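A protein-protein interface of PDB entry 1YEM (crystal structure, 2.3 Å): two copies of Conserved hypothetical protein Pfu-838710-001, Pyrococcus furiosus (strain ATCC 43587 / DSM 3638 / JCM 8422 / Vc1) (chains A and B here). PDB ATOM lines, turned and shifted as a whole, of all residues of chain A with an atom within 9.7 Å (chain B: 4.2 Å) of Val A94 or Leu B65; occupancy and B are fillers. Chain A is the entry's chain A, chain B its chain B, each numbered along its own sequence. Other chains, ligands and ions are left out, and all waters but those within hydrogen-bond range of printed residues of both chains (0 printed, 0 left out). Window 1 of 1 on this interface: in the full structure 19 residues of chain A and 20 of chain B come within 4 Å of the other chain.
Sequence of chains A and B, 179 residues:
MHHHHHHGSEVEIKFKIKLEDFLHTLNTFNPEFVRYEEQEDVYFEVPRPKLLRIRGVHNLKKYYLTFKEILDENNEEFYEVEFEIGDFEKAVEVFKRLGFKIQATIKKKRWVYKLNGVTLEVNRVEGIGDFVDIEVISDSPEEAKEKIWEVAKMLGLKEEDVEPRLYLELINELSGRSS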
ATOM      1  N   PHE A  44      37.030  -0.568  30.944  1.00  0.00           N
ATOM      2  CA  PHE A  44      37.628  -1.522  30.033  1.00  0.00           C
ATOM      3  C   PHE A  44      39.137  -1.310  30.007  1.00  0.00           C
ATOM      4  O   PHE A  44      39.612  -0.165  30.117  1.00  0.00           O
ATOM      5  CB  PHE A  44      37.019  -1.397  28.637  1.00  0.00           C
ATOM      6  CG  PHE A  44      35.599  -1.851  28.573  1.00  0.00           C
ATOM      7  CD1 PHE A  44      35.293  -3.186  28.344  1.00  0.00           C
ATOM      8  CD2 PHE A  44      34.551  -0.944  28.784  1.00  0.00           C
ATOM      9  CE1 PHE A  44      33.987  -3.609  28.300  1.00  0.00           C
ATOM     10  CE2 PHE A  44      33.240  -1.363  28.759  1.00  0.00           C
ATOM     11  CZ  PHE A  44      32.949  -2.688  28.516  1.00  0.00           C
ATOM     12  N   LEU A  52      38.705   4.255  29.807  1.00  0.00           N
ATOM     13  CA  LEU A  52      37.497   4.069  29.038  1.00  0.00           C
ATOM     14  C   LEU A  52      36.457   3.402  29.916  1.00  0.00           C
ATOM     15  O   LEU A  52      36.669   2.292  30.398  1.00  0.00           O
ATOM     16  CB  LEU A  52      37.779   3.204  27.812  1.00  0.00           C
ATOM     17  CG  LEU A  52      36.592   2.825  26.931  1.00  0.00           C
ATOM     18  CD1 LEU A  52      35.997   4.041  26.259  1.00  0.00           C
ATOM     19  CD2 LEU A  52      37.039   1.807  25.879  1.00  0.00           C
ATOM     20  N   ILE A  54      31.972   2.961  30.738  1.00  0.00           N
ATOM     21  CA  ILE A  54      30.587   3.160  30.520  1.00  0.00           C
ATOM     22  C   ILE A  54      29.987   3.378  31.886  1.00  0.00           C
ATOM     23  O   ILE A  54      30.189   2.556  32.807  1.00  0.00           O
ATOM     24  CB  ILE A  54      29.987   1.943  29.815  1.00  0.00           C
ATOM     25  CG1 ILE A  54      30.634   1.807  28.424  1.00  0.00           C
ATOM     26  CG2 ILE A  54      28.477   2.089  29.681  1.00  0.00           C
ATOM     27  CD1 ILE A  54      30.376   0.503  27.774  1.00  0.00           C
ATOM     28  N   LEU A  65      29.208   7.270  27.922  1.00  0.00           N
ATOM     29  CA  LEU A  65      30.467   6.675  27.609  1.00  0.00           C
ATOM     30  C   LEU A  65      31.505   7.754  27.845  1.00  0.00           C
ATOM     31  O   LEU A  65      31.364   8.886  27.352  1.00  0.00           O
ATOM     32  CB  LEU A  65      30.491   6.182  26.165  1.00  0.00           C
ATOM     33  CG  LEU A  65      31.838   5.581  25.716  1.00  0.00           C
ATOM     34  CD1 LEU A  65      31.625   4.677  24.554  1.00  0.00           C
ATOM     35  CD2 LEU A  65      32.856   6.662  25.369  1.00  0.00           C
ATOM     36  N   PHE A  83      29.913  11.436  26.064  1.00  0.00           N
ATOM     37  CA  PHE A  83      28.600  11.713  25.494  1.00  0.00           C
ATOM     38  C   PHE A  83      27.606  10.687  26.061  1.00  0.00           C
ATOM     39  O   PHE A  83      28.020   9.620  26.568  1.00  0.00           O
ATOM     40  CB  PHE A  83      28.676  11.636  23.950  1.00  0.00           C
ATOM     41  CG  PHE A  83      29.354  10.381  23.435  1.00  0.00           C
ATOM     42  CD1 PHE A  83      28.627   9.224  23.226  1.00  0.00           C
ATOM     43  CD2 PHE A  83      30.736  10.365  23.197  1.00  0.00           C
ATOM     44  CE1 PHE A  83      29.252   8.052  22.765  1.00  0.00           C
ATOM     45  CE2 PHE A  83      31.378   9.222  22.746  1.00  0.00           C
ATOM     46  CZ  PHE A  83      30.641   8.053  22.526  1.00  0.00           C
ATOM     47  N   GLU A  84      26.310  11.022  25.990  1.00  0.00           N
ATOM     48  CA  GLU A  84      25.243  10.117  26.427  1.00  0.00           C
ATOM     49  C   GLU A  84      25.068   8.970  25.470  1.00  0.00           C
ATOM     50  O   GLU A  84      25.292   9.096  24.294  1.00  0.00           O
ATOM     51  CB  GLU A  84      23.900  10.834  26.522  1.00  0.00           C
ATOM     52  CG  GLU A  84      23.663  11.553  27.805  1.00  0.00           C
ATOM     53  CD  GLU A  84      22.233  12.055  27.920  1.00  0.00           C
ATOM     54  OE1 GLU A  84      22.046  13.293  27.847  1.00  0.00           O
ATOM     55  OE2 GLU A  84      21.306  11.215  28.075  1.00  0.00           O
ATOM     56  N   ILE A  85      24.666   7.846  26.006  1.00  0.00           N
ATOM     57  CA  ILE A  85      24.327   6.678  25.229  1.00  0.00           C
ATOM     58  C   ILE A  85      22.938   6.251  25.697  1.00  0.00           C
ATOM     59  O   ILE A  85      22.541   6.586  26.800  1.00  0.00           O
ATOM     60  CB  ILE A  85      25.358   5.537  25.435  1.00  0.00           C
ATOM     61  CG1 ILE A  85      25.301   4.973  26.862  1.00  0.00           C
ATOM     62  CG2 ILE A  85      26.762   6.041  25.129  1.00  0.00           C
ATOM     63  CD1 ILE A  85      26.329   3.927  27.142  1.00  0.00           C
ATOM     64  N   GLY A  86      22.204   5.516  24.872  1.00  0.00           N
ATOM     65  CA  GLY A  86      20.811   5.180  25.201  1.00  0.00           C
ATOM     66  C   GLY A  86      20.630   3.860  25.904  1.00  0.00           C
ATOM     67  O   GLY A  86      19.553   3.568  26.383  1.00  0.00           O
ATOM     68  N   ASP A  87      21.671   3.044  25.966  1.00  0.00           N
ATOM     69  CA  ASP A  87      21.536   1.710  26.530  1.00  0.00           C
ATOM     70  C   ASP A  87      22.847   1.235  27.132  1.00  0.00           C
ATOM     71  O   ASP A  87      23.813   0.955  26.412  1.00  0.00           O
ATOM     72  CB  ASP A  87      21.049   0.728  25.454  1.00  0.00           C
ATOM     73  CG  ASP A  87      20.567  -0.588  26.036  1.00  0.00           C
ATOM     74  OD1 ASP A  87      19.436  -1.010  25.720  1.00  0.00           O
ATOM     75  OD2 ASP A  87      21.304  -1.207  26.809  1.00  0.00           O
ATOM     76  N   PHE A  88      22.850   1.117  28.457  1.00  0.00           N
ATOM     77  CA  PHE A  88      24.028   0.743  29.229  1.00  0.00           C
ATOM     78  C   PHE A  88      24.554  -0.633  28.859  1.00  0.00           C
ATOM     79  O   PHE A  88      25.713  -0.774  28.498  1.00  0.00           O
ATOM     80  CB  PHE A  88      23.703   0.819  30.736  1.00  0.00           C
ATOM     81  CG  PHE A  88      24.842   0.400  31.636  1.00  0.00           C
ATOM     82  CD1 PHE A  88      25.855   1.295  31.963  1.00  0.00           C
ATOM     83  CD2 PHE A  88      24.890  -0.878  32.166  1.00  0.00           C
ATOM     84  CE1 PHE A  88      26.893   0.931  32.792  1.00  0.00           C
ATOM     85  CE2 PHE A  88      25.932  -1.254  33.001  1.00  0.00           C
ATOM     86  CZ  PHE A  88      26.943  -0.330  33.311  1.00  0.00           C
ATOM     87  N   GLU A  89      23.695  -1.641  28.943  1.00  0.00           N
ATOM     88  CA  GLU A  89      24.099  -3.017  28.681  1.00  0.00           C
ATOM     89  C   GLU A  89      24.549  -3.246  27.230  1.00  0.00           C
ATOM     90  O   GLU A  89      25.525  -3.953  26.986  1.00  0.00           O
ATOM     91  CB  GLU A  89      22.974  -3.992  29.059  1.00  0.00           C
ATOM     92  CG  GLU A  89      22.692  -4.087  30.595  1.00  0.00           C
ATOM     93  CD  GLU A  89      23.928  -4.522  31.463  1.00  0.00           C
ATOM     94  OE1 GLU A  89      23.930  -4.216  32.688  1.00  0.00           O
ATOM     95  OE2 GLU A  89      24.884  -5.158  30.934  1.00  0.00           O
ATOM     96  N   LYS A  90      23.855  -2.646  26.271  1.00  0.00           N
ATOM     97  CA  LYS A  90      24.253  -2.802  24.865  1.00  0.00           C
ATOM     98  C   LYS A  90      25.646  -2.219  24.618  1.00  0.00           C
ATOM     99  O   LYS A  90      26.445  -2.816  23.918  1.00  0.00           O
ATOM    100  CB  LYS A  90      23.236  -2.161  23.927  1.00  0.00           C
ATOM    101  CG  LYS A  90      21.926  -2.930  23.805  1.00  0.00           C
ATOM    102  CD  LYS A  90      21.032  -2.283  22.756  1.00  0.00           C
ATOM    103  CE  LYS A  90      19.807  -3.115  22.477  1.00  0.00           C
ATOM    104  NZ  LYS A  90      19.077  -2.608  21.265  1.00  0.00           N
ATOM    105  N   ALA A  91      25.930  -1.059  25.209  1.00  0.00           N
ATOM    106  CA  ALA A  91      27.259  -0.439  25.090  1.00  0.00           C
ATOM    107  C   ALA A  91      28.349  -1.340  25.675  1.00  0.00           C
ATOM    108  O   ALA A  91      29.418  -1.508  25.065  1.00  0.00           O
ATOM    109  CB  ALA A  91      27.274   0.893  25.740  1.00  0.00           C
ATOM    110  N   VAL A  92      28.066  -1.948  26.835  1.00  0.00           N
ATOM    111  CA  VAL A  92      28.975  -2.936  27.418  1.00  0.00           C
ATOM    112  C   VAL A  92      29.131  -4.116  26.459  1.00  0.00           C
ATOM    113  O   VAL A  92      30.234  -4.588  26.240  1.00  0.00           O
ATOM    114  CB  VAL A  92      28.514  -3.444  28.836  1.00  0.00           C
ATOM    115  CG1 VAL A  92      29.442  -4.537  29.340  1.00  0.00           C
ATOM    116  CG2 VAL A  92      28.483  -2.301  29.859  1.00  0.00           C
ATOM    117  N   GLU A  93      28.037  -4.566  25.860  1.00  0.00           N
ATOM    118  CA  GLU A  93      28.106  -5.691  24.917  1.00  0.00           C
ATOM    119  C   GLU A  93      28.966  -5.359  23.685  1.00  0.00           C
ATOM    120  O   GLU A  93      29.805  -6.147  23.278  1.00  0.00           O
ATOM    121  CB  GLU A  93      26.707  -6.110  24.492  1.00  0.00           C
ATOM    122  CG  GLU A  93      26.686  -7.354  23.645  1.00  0.00           C
ATOM    123  CD  GLU A  93      25.308  -7.677  23.122  1.00  0.00           C
ATOM    124  OE1 GLU A  93      24.310  -7.153  23.691  1.00  0.00           O
ATOM    125  OE2 GLU A  93      25.225  -8.453  22.134  1.00  0.00           O
ATOM    126  N   VAL A  94      28.772  -4.183  23.110  1.00  0.00           N
ATOM    127  CA  VAL A  94      29.543  -3.799  21.932  1.00  0.00           C
ATOM    128  C   VAL A  94      31.029  -3.840  22.230  1.00  0.00           C
ATOM    129  O   VAL A  94      31.782  -4.461  21.500  1.00  0.00           O
ATOM    130  CB  VAL A  94      29.144  -2.405  21.401  1.00  0.00           C
ATOM    131  CG1 VAL A  94      30.138  -1.920  20.358  1.00  0.00           C
ATOM    132  CG2 VAL A  94      27.739  -2.449  20.808  1.00  0.00           C
ATOM    133  N   PHE A  95      31.451  -3.196  23.314  1.00  0.00           N
ATOM    134  CA  PHE A  95      32.885  -3.160  23.660  1.00  0.00           C
ATOM    135  C   PHE A  95      33.478  -4.531  23.975  1.00  0.00           C
ATOM    136  O   PHE A  95      34.631  -4.790  23.635  1.00  0.00           O
ATOM    137  CB  PHE A  95      33.173  -2.132  24.776  1.00  0.00           C
ATOM    138  CG  PHE A  95      33.248  -0.733  24.264  1.00  0.00           C
ATOM    139  CD1 PHE A  95      32.139   0.097  24.301  1.00  0.00           C
ATOM    140  CD2 PHE A  95      34.412  -0.272  23.654  1.00  0.00           C
ATOM    141  CE1 PHE A  95      32.197   1.396  23.787  1.00  0.00           C
ATOM    142  CE2 PHE A  95      34.477   1.018  23.127  1.00  0.00           C
ATOM    143  CZ  PHE A  95      33.364   1.857  23.206  1.00  0.00           C
ATOM    144  N   LYS A  96      32.696  -5.414  24.593  1.00  0.00           N
ATOM    145  CA  LYS A  96      33.138  -6.798  24.776  1.00  0.00           C
ATOM    146  C   LYS A  96      33.351  -7.462  23.414  1.00  0.00           C
ATOM    147  O   LYS A  96      34.393  -8.061  23.164  1.00  0.00           O
ATOM    148  CB  LYS A  96      32.135  -7.618  25.602  1.00  0.00           C
ATOM    149  CG  LYS A  96      32.113  -7.303  27.117  1.00  0.00           C
ATOM    150  CD  LYS A  96      31.591  -8.503  27.933  1.00  0.00           C
ATOM    151  CE  LYS A  96      30.684  -8.090  29.089  1.00  0.00           C
ATOM    152  NZ  LYS A  96      29.221  -7.935  28.665  1.00  0.00           N
ATOM    153  N   ARG A  97      32.370  -7.332  22.528  1.00  0.00           N
ATOM    154  CA  ARG A  97      32.446  -7.976  21.212  1.00  0.00           C
ATOM    155  C   ARG A  97      33.539  -7.417  20.325  1.00  0.00           C
ATOM    156  O   ARG A  97      33.961  -8.078  19.392  1.00  0.00           O
ATOM    157  CB  ARG A  97      31.102  -7.921  20.494  1.00  0.00           C
ATOM    158  CG  ARG A  97      30.132  -8.931  21.036  1.00  0.00           C
ATOM    159  CD  ARG A  97      28.832  -8.875  20.319  1.00  0.00           C
ATOM    160  NE  ARG A  97      27.809  -9.666  20.998  1.00  0.00           N
ATOM    161  CZ  ARG A  97      27.702 -10.992  20.923  1.00  0.00           C
ATOM    162  NH1 ARG A  97      28.568 -11.715  20.211  1.00  0.00           N
ATOM    163  NH2 ARG A  97      26.724 -11.606  21.582  1.00  0.00           N
ATOM    164  N   LEU A  98      34.010  -6.214  20.626  1.00  0.00           N
ATOM    165  CA  LEU A  98      35.169  -5.666  19.937  1.00  0.00           C
ATOM    166  C   LEU A  98      36.481  -6.164  20.541  1.00  0.00           C
ATOM    167  O   LEU A  98      37.540  -5.824  20.052  1.00  0.00           O
ATOM    168  CB  LEU A  98      35.119  -4.143  19.951  1.00  0.00           C
ATOM    169  CG  LEU A  98      33.940  -3.536  19.176  1.00  0.00           C
ATOM    170  CD1 LEU A  98      33.675  -2.099  19.615  1.00  0.00           C
ATOM    171  CD2 LEU A  98      34.193  -3.613  17.654  1.00  0.00           C
ATOM    172  N   GLY A  99      36.407  -6.959  21.604  1.00  0.00           N
ATOM    173  CA  GLY A  99      37.607  -7.556  22.209  1.00  0.00           C
ATOM    174  C   GLY A  99      38.150  -6.838  23.440  1.00  0.00           C
ATOM    175  O   GLY A  99      39.202  -7.222  23.958  1.00  0.00           O
ATOM    176  N   PHE A 100      37.450  -5.804  23.921  1.00  0.00           N
ATOM    177  CA  PHE A 100      37.864  -5.134  25.160  1.00  0.00           C
ATOM    178  C   PHE A 100      37.486  -5.969  26.370  1.00  0.00           C
ATOM    179  O   PHE A 100      36.446  -6.649  26.367  1.00  0.00           O
ATOM    180  CB  PHE A 100      37.270  -3.740  25.272  1.00  0.00           C
ATOM    181  CG  PHE A 100      37.855  -2.763  24.295  1.00  0.00           C
ATOM    182  CD1 PHE A 100      38.967  -2.009  24.630  1.00  0.00           C
ATOM    183  CD2 PHE A 100      37.292  -2.597  23.035  1.00  0.00           C
ATOM    184  CE1 PHE A 100      39.506  -1.089  23.735  1.00  0.00           C
ATOM    185  CE2 PHE A 100      37.827  -1.682  22.131  1.00  0.00           C
ATOM    186  CZ  PHE A 100      38.937  -0.930  22.488  1.00  0.00           C
ATOM    187  N   LYS A 101      38.361  -5.935  27.385  1.00  0.00           N
ATOM    188  CA  LYS A 101      38.149  -6.656  28.643  1.00  0.00           C
ATOM    189  C   LYS A 101      37.738  -5.679  29.754  1.00  0.00           C
ATOM    190  O   LYS A 101      38.299  -4.582  29.876  1.00  0.00           O
ATOM    191  CB  LYS A 101      39.425  -7.397  29.061  1.00  0.00           C
ATOM    192  CG  LYS A 101      40.004  -8.352  27.995  1.00  0.00           C
ATOM    193  CD  LYS A 101      39.075  -9.562  27.724  1.00  0.00           C
ATOM    194  N   ARG B  53      30.226   0.955  13.126  1.00  0.00           N
ATOM    195  CA  ARG B  53      29.986   2.260  12.518  1.00  0.00           C
ATOM    196  C   ARG B  53      29.231   3.218  13.417  1.00  0.00           C
ATOM    197  O   ARG B  53      28.423   2.809  14.269  1.00  0.00           O
ATOM    198  CB  ARG B  53      29.230   2.131  11.176  1.00  0.00           C
ATOM    199  CG  ARG B  53      27.787   1.696  11.285  1.00  0.00           C
ATOM    200  CD  ARG B  53      26.906   2.349  10.243  1.00  0.00           C
ATOM    201  NE  ARG B  53      26.005   1.357   9.665  1.00  0.00           N
ATOM    202  CZ  ARG B  53      24.889   0.904  10.230  1.00  0.00           C
ATOM    203  NH1 ARG B  53      24.462   1.366  11.392  1.00  0.00           N
ATOM    204  NH2 ARG B  53      24.181  -0.005   9.605  1.00  0.00           N
ATOM    205  N   ILE B  54      29.514   4.499  13.208  1.00  0.00           N
ATOM    206  CA  ILE B  54      28.781   5.585  13.828  1.00  0.00           C
ATOM    207  C   ILE B  54      27.922   6.195  12.730  1.00  0.00           C
ATOM    208  O   ILE B  54      28.421   6.517  11.657  1.00  0.00           O
ATOM    209  CB  ILE B  54      29.725   6.677  14.417  1.00  0.00           C
ATOM    210  CG1 ILE B  54      30.793   6.047  15.340  1.00  0.00           C
ATOM    211  CG2 ILE B  54      28.936   7.728  15.171  1.00  0.00           C
ATOM    212  CD1 ILE B  54      30.263   5.092  16.375  1.00  0.00           C
ATOM    213  N   TYR B  64      23.809   7.223  16.186  1.00  0.00           N
ATOM    214  CA  TYR B  64      23.798   5.834  16.596  1.00  0.00           C
ATOM    215  C   TYR B  64      25.161   5.251  16.496  1.00  0.00           C
ATOM    216  O   TYR B  64      25.950   5.670  15.690  1.00  0.00           O
ATOM    217  CB  TYR B  64      22.852   5.017  15.709  1.00  0.00           C
ATOM    218  CG  TYR B  64      21.465   5.564  15.721  1.00  0.00           C
ATOM    219  CD1 TYR B  64      21.091   6.564  14.830  1.00  0.00           C
ATOM    220  CD2 TYR B  64      20.527   5.109  16.646  1.00  0.00           C
ATOM    221  CE1 TYR B  64      19.809   7.095  14.846  1.00  0.00           C
ATOM    222  CE2 TYR B  64      19.243   5.626  16.676  1.00  0.00           C
ATOM    223  CZ  TYR B  64      18.890   6.627  15.769  1.00  0.00           C
ATOM    224  OH  TYR B  64      17.631   7.168  15.787  1.00  0.00           O
ATOM    225  N   LEU B  65      25.412   4.278  17.348  1.00  0.00           N
ATOM    226  CA  LEU B  65      26.576   3.446  17.276  1.00  0.00           C
ATOM    227  C   LEU B  65      26.067   2.049  16.993  1.00  0.00           C
ATOM    228  O   LEU B  65      25.177   1.564  17.688  1.00  0.00           O
ATOM    229  CB  LEU B  65      27.330   3.480  18.596  1.00  0.00           C
ATOM    230  CG  LEU B  65      28.674   2.728  18.632  1.00  0.00           C
ATOM    231  CD1 LEU B  65      29.622   3.367  19.647  1.00  0.00           C
ATOM    232  CD2 LEU B  65      28.483   1.235  18.942  1.00  0.00           C
ATOM    233  N   THR B  66      26.612   1.416  15.956  1.00  0.00           N
ATOM    234  CA  THR B  66      26.142   0.099  15.532  1.00  0.00           C
ATOM    235  C   THR B  66      27.301  -0.886  15.413  1.00  0.00           C
ATOM    236  O   THR B  66      28.343  -0.566  14.849  1.00  0.00           O
ATOM    237  CB  THR B  66      25.414   0.183  14.177  1.00  0.00           C
ATOM    238  OG1 THR B  66      24.363   1.158  14.256  1.00  0.00           O
ATOM    239  CG2 THR B  66      24.817  -1.166  13.791  1.00  0.00           C
ATOM    240  N   PHE B  67      27.115  -2.066  15.984  1.00  0.00           N
ATOM    241  CA  PHE B  67      28.043  -3.176  15.802  1.00  0.00           C
ATOM    242  C   PHE B  67      27.276  -4.325  15.157  1.00  0.00           C
ATOM    243  O   PHE B  67      26.174  -4.622  15.577  1.00  0.00           O
ATOM    244  CB  PHE B  67      28.637  -3.626  17.146  1.00  0.00           C
ATOM    245  CG  PHE B  67      29.346  -4.940  17.079  1.00  0.00           C
ATOM    246  CD1 PHE B  67      30.694  -5.003  16.769  1.00  0.00           C
ATOM    247  CD2 PHE B  67      28.656  -6.130  17.299  1.00  0.00           C
ATOM    248  CE1 PHE B  67      31.344  -6.235  16.680  1.00  0.00           C
ATOM    249  CE2 PHE B  67      29.297  -7.352  17.213  1.00  0.00           C
ATOM    250  CZ  PHE B  67      30.637  -7.409  16.908  1.00  0.00           C
ATOM    251  N   VAL B  81      23.963  -5.131  17.225  1.00  0.00           N
ATOM    252  CA  VAL B  81      23.707  -4.394  18.465  1.00  0.00           C
ATOM    253  C   VAL B  81      23.858  -2.906  18.175  1.00  0.00           C
ATOM    254  O   VAL B  81      24.910  -2.469  17.684  1.00  0.00           O
ATOM    255  CB  VAL B  81      24.701  -4.760  19.614  1.00  0.00           C
ATOM    256  CG1 VAL B  81      24.217  -4.159  20.923  1.00  0.00           C
ATOM    257  CG2 VAL B  81      24.841  -6.246  19.757  1.00  0.00           C
ATOM    258  N   GLU B  82      22.827  -2.127  18.476  1.00  0.00           N
ATOM    259  CA  GLU B  82      22.933  -0.688  18.330  1.00  0.00           C
ATOM    260  C   GLU B  82      22.174   0.110  19.397  1.00  0.00           C
ATOM    261  O   GLU B  82      21.229  -0.364  20.019  1.00  0.00           O
ATOM    262  CB  GLU B  82      22.526  -0.255  16.915  1.00  0.00           C
ATOM    263  CG  GLU B  82      21.096   0.113  16.721  1.00  0.00           C
ATOM    264  CD  GLU B  82      20.833   0.704  15.336  1.00  0.00           C
ATOM    265  OE1 GLU B  82      21.728   0.633  14.449  1.00  0.00           O
ATOM    266  OE2 GLU B  82      19.719   1.247  15.130  1.00  0.00           O
ATOM    267  N   PHE B  83      22.634   1.328  19.605  1.00  0.00           N
ATOM    268  CA  PHE B  83      22.011   2.233  20.547  1.00  0.00           C
ATOM    269  C   PHE B  83      22.305   3.642  20.104  1.00  0.00           C
ATOM    270  O   PHE B  83      23.258   3.902  19.354  1.00  0.00           O
ATOM    271  CB  PHE B  83      22.534   2.003  21.986  1.00  0.00           C
ATOM    272  CG  PHE B  83      24.036   1.994  22.098  1.00  0.00           C
ATOM    273  CD1 PHE B  83      24.726   3.141  22.391  1.00  0.00           C
ATOM    274  CD2 PHE B  83      24.752   0.821  21.899  1.00  0.00           C
ATOM    275  CE1 PHE B  83      26.128   3.135  22.477  1.00  0.00           C
ATOM    276  CE2 PHE B  83      26.136   0.803  22.003  1.00  0.00           C
ATOM    277  CZ  PHE B  83      26.822   1.963  22.289  1.00  0.00           C
ATOM    278  N   ILE B  85      23.413   7.532  20.504  1.00  0.00           N
ATOM    279  CA  ILE B  85      24.423   8.315  21.181  1.00  0.00           C
ATOM    280  C   ILE B  85      24.066   9.799  21.062  1.00  0.00           C
ATOM    281  O   ILE B  85      23.274  10.197  20.190  1.00  0.00           O
ATOM    282  CB  ILE B  85      25.844   8.039  20.632  1.00  0.00           C
ATOM    283  CG1 ILE B  85      25.970   8.534  19.191  1.00  0.00           C
ATOM    284  CG2 ILE B  85      26.157   6.558  20.752  1.00  0.00           C
ATOM    285  CD1 ILE B  85      27.218   8.062  18.452  1.00  0.00           C
ATOM    286  N   PHE B  95      36.823   6.850  19.178  1.00  0.00           N
ATOM    287  CA  PHE B  95      37.284   5.640  18.482  1.00  0.00           C
ATOM    288  C   PHE B  95      38.635   5.814  17.770  1.00  0.00           C
ATOM    289  O   PHE B  95      39.471   4.921  17.823  1.00  0.00           O
ATOM    290  CB  PHE B  95      36.199   5.099  17.530  1.00  0.00           C
ATOM    291  CG  PHE B  95      35.222   4.236  18.217  1.00  0.00           C
ATOM    292  CD1 PHE B  95      34.004   4.732  18.624  1.00  0.00           C
ATOM    293  CD2 PHE B  95      35.557   2.937  18.545  1.00  0.00           C
ATOM    294  CE1 PHE B  95      33.105   3.925  19.317  1.00  0.00           C
ATOM    295  CE2 PHE B  95      34.671   2.122  19.238  1.00  0.00           C
ATOM    296  CZ  PHE B  95      33.440   2.613  19.618  1.00  0.00           C
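Phe A83 touches Ile B85, and with the chains exchanged Ile A85 touches Phe B83.
Phe A95 touches its own counterpart, Phe B95.
5 positions are printed for both chains.
The side-chain carboxylate (OD2) of Asp A87 is in hydrogen-bond range of the backbone NH (N) of Glu A89, 3.2 Å away.
The guanidinium group (NE) of Arg A97 lies within salt-bridge range of the side-chain carboxylate (OE2) of Glu A93 (3.1 Å).
The backbone NH of Leu A65 is in hydrogen-bond range of the backbone carbonyl oxygen of Phe A83 (3.0 Å).
The backbone carbonyl oxygen (O) of Phe A95 sits at hydrogen-bond distance from the backbone NH (N) of Phe A100 (3.0 Å).
The side-chain carboxylate of Asp A87 is in hydrogen-bond range of the backbone NH of Lys A90.
The side-chain carboxylate (OE1) of Glu B82 lies within hydrogen-bond range of the side-chain hydroxyl (OG1) of Thr B66 (2.7 Å).
The backbone carbonyl oxygen of Glu B82 lies close to the side-chain amino group of Lys A90 (3.3 Å).
Of the 11 printed residues of chain B, 7 touch a printed residue of chain A.
Hydrophobic or aromatic side chains of chain B that line the printed part of chain A: Leu B65, Phe B67, Val B81, Phe B83, Ile B85 and Phe B95.
Of the 23 printed residues of chain A, 11 touch a printed residue of chain B.
Among the printed residues, no Asp or Glu carboxylate lies within 4 Å of a Lys or Arg side-chain nitrogen of the other chain.
Ile A85 touches Phe B83 (CB to CE1, 3.9 Å).
CB of Asp A87 touches CB of Phe B83, at 3.98 Å.
Lys A90 touches Val B81.
Lys A90 touches Phe B83.
CB of Phe B67 touches CG1 of Val A94 (3.9 Å).
CG2 of Val A94 touches CG1 of Val B81 (3.9 Å).
Phe B83 touches Val A94.
Phe B95 touches Phe A95 (CZ to CZ, 3.7 Å).
CD of Arg A97 touches CE2 of Phe B67, 3.5 Å away.
Phe B67 touches Leu A98.
Of chain B, only Leu B65 (3.8 Å), Phe B67 (3.9 Å), Val B81 (3.9 Å) and Phe B83 (3.8 Å) come within 4 Å of Val A94.
Leu B65 touches just one residue of chain A: Val A94 (3.8 Å).
Printed residues of chain B within 4 Å of Ile A85: Phe B83.
Of the printed residues of chain A, Phe B67 touches Val A94 (3.9 Å), Arg A97 (3.5 Å) and Leu A98 (3.9 Å).
Of the printed residues of chain A, Glu B82 touches Lys A90 (3.3 Å).
Printed residues of chain B within 4 Å of Phe A83: Ile B85.
Leu A52 touches none of the printed residues of chain B.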
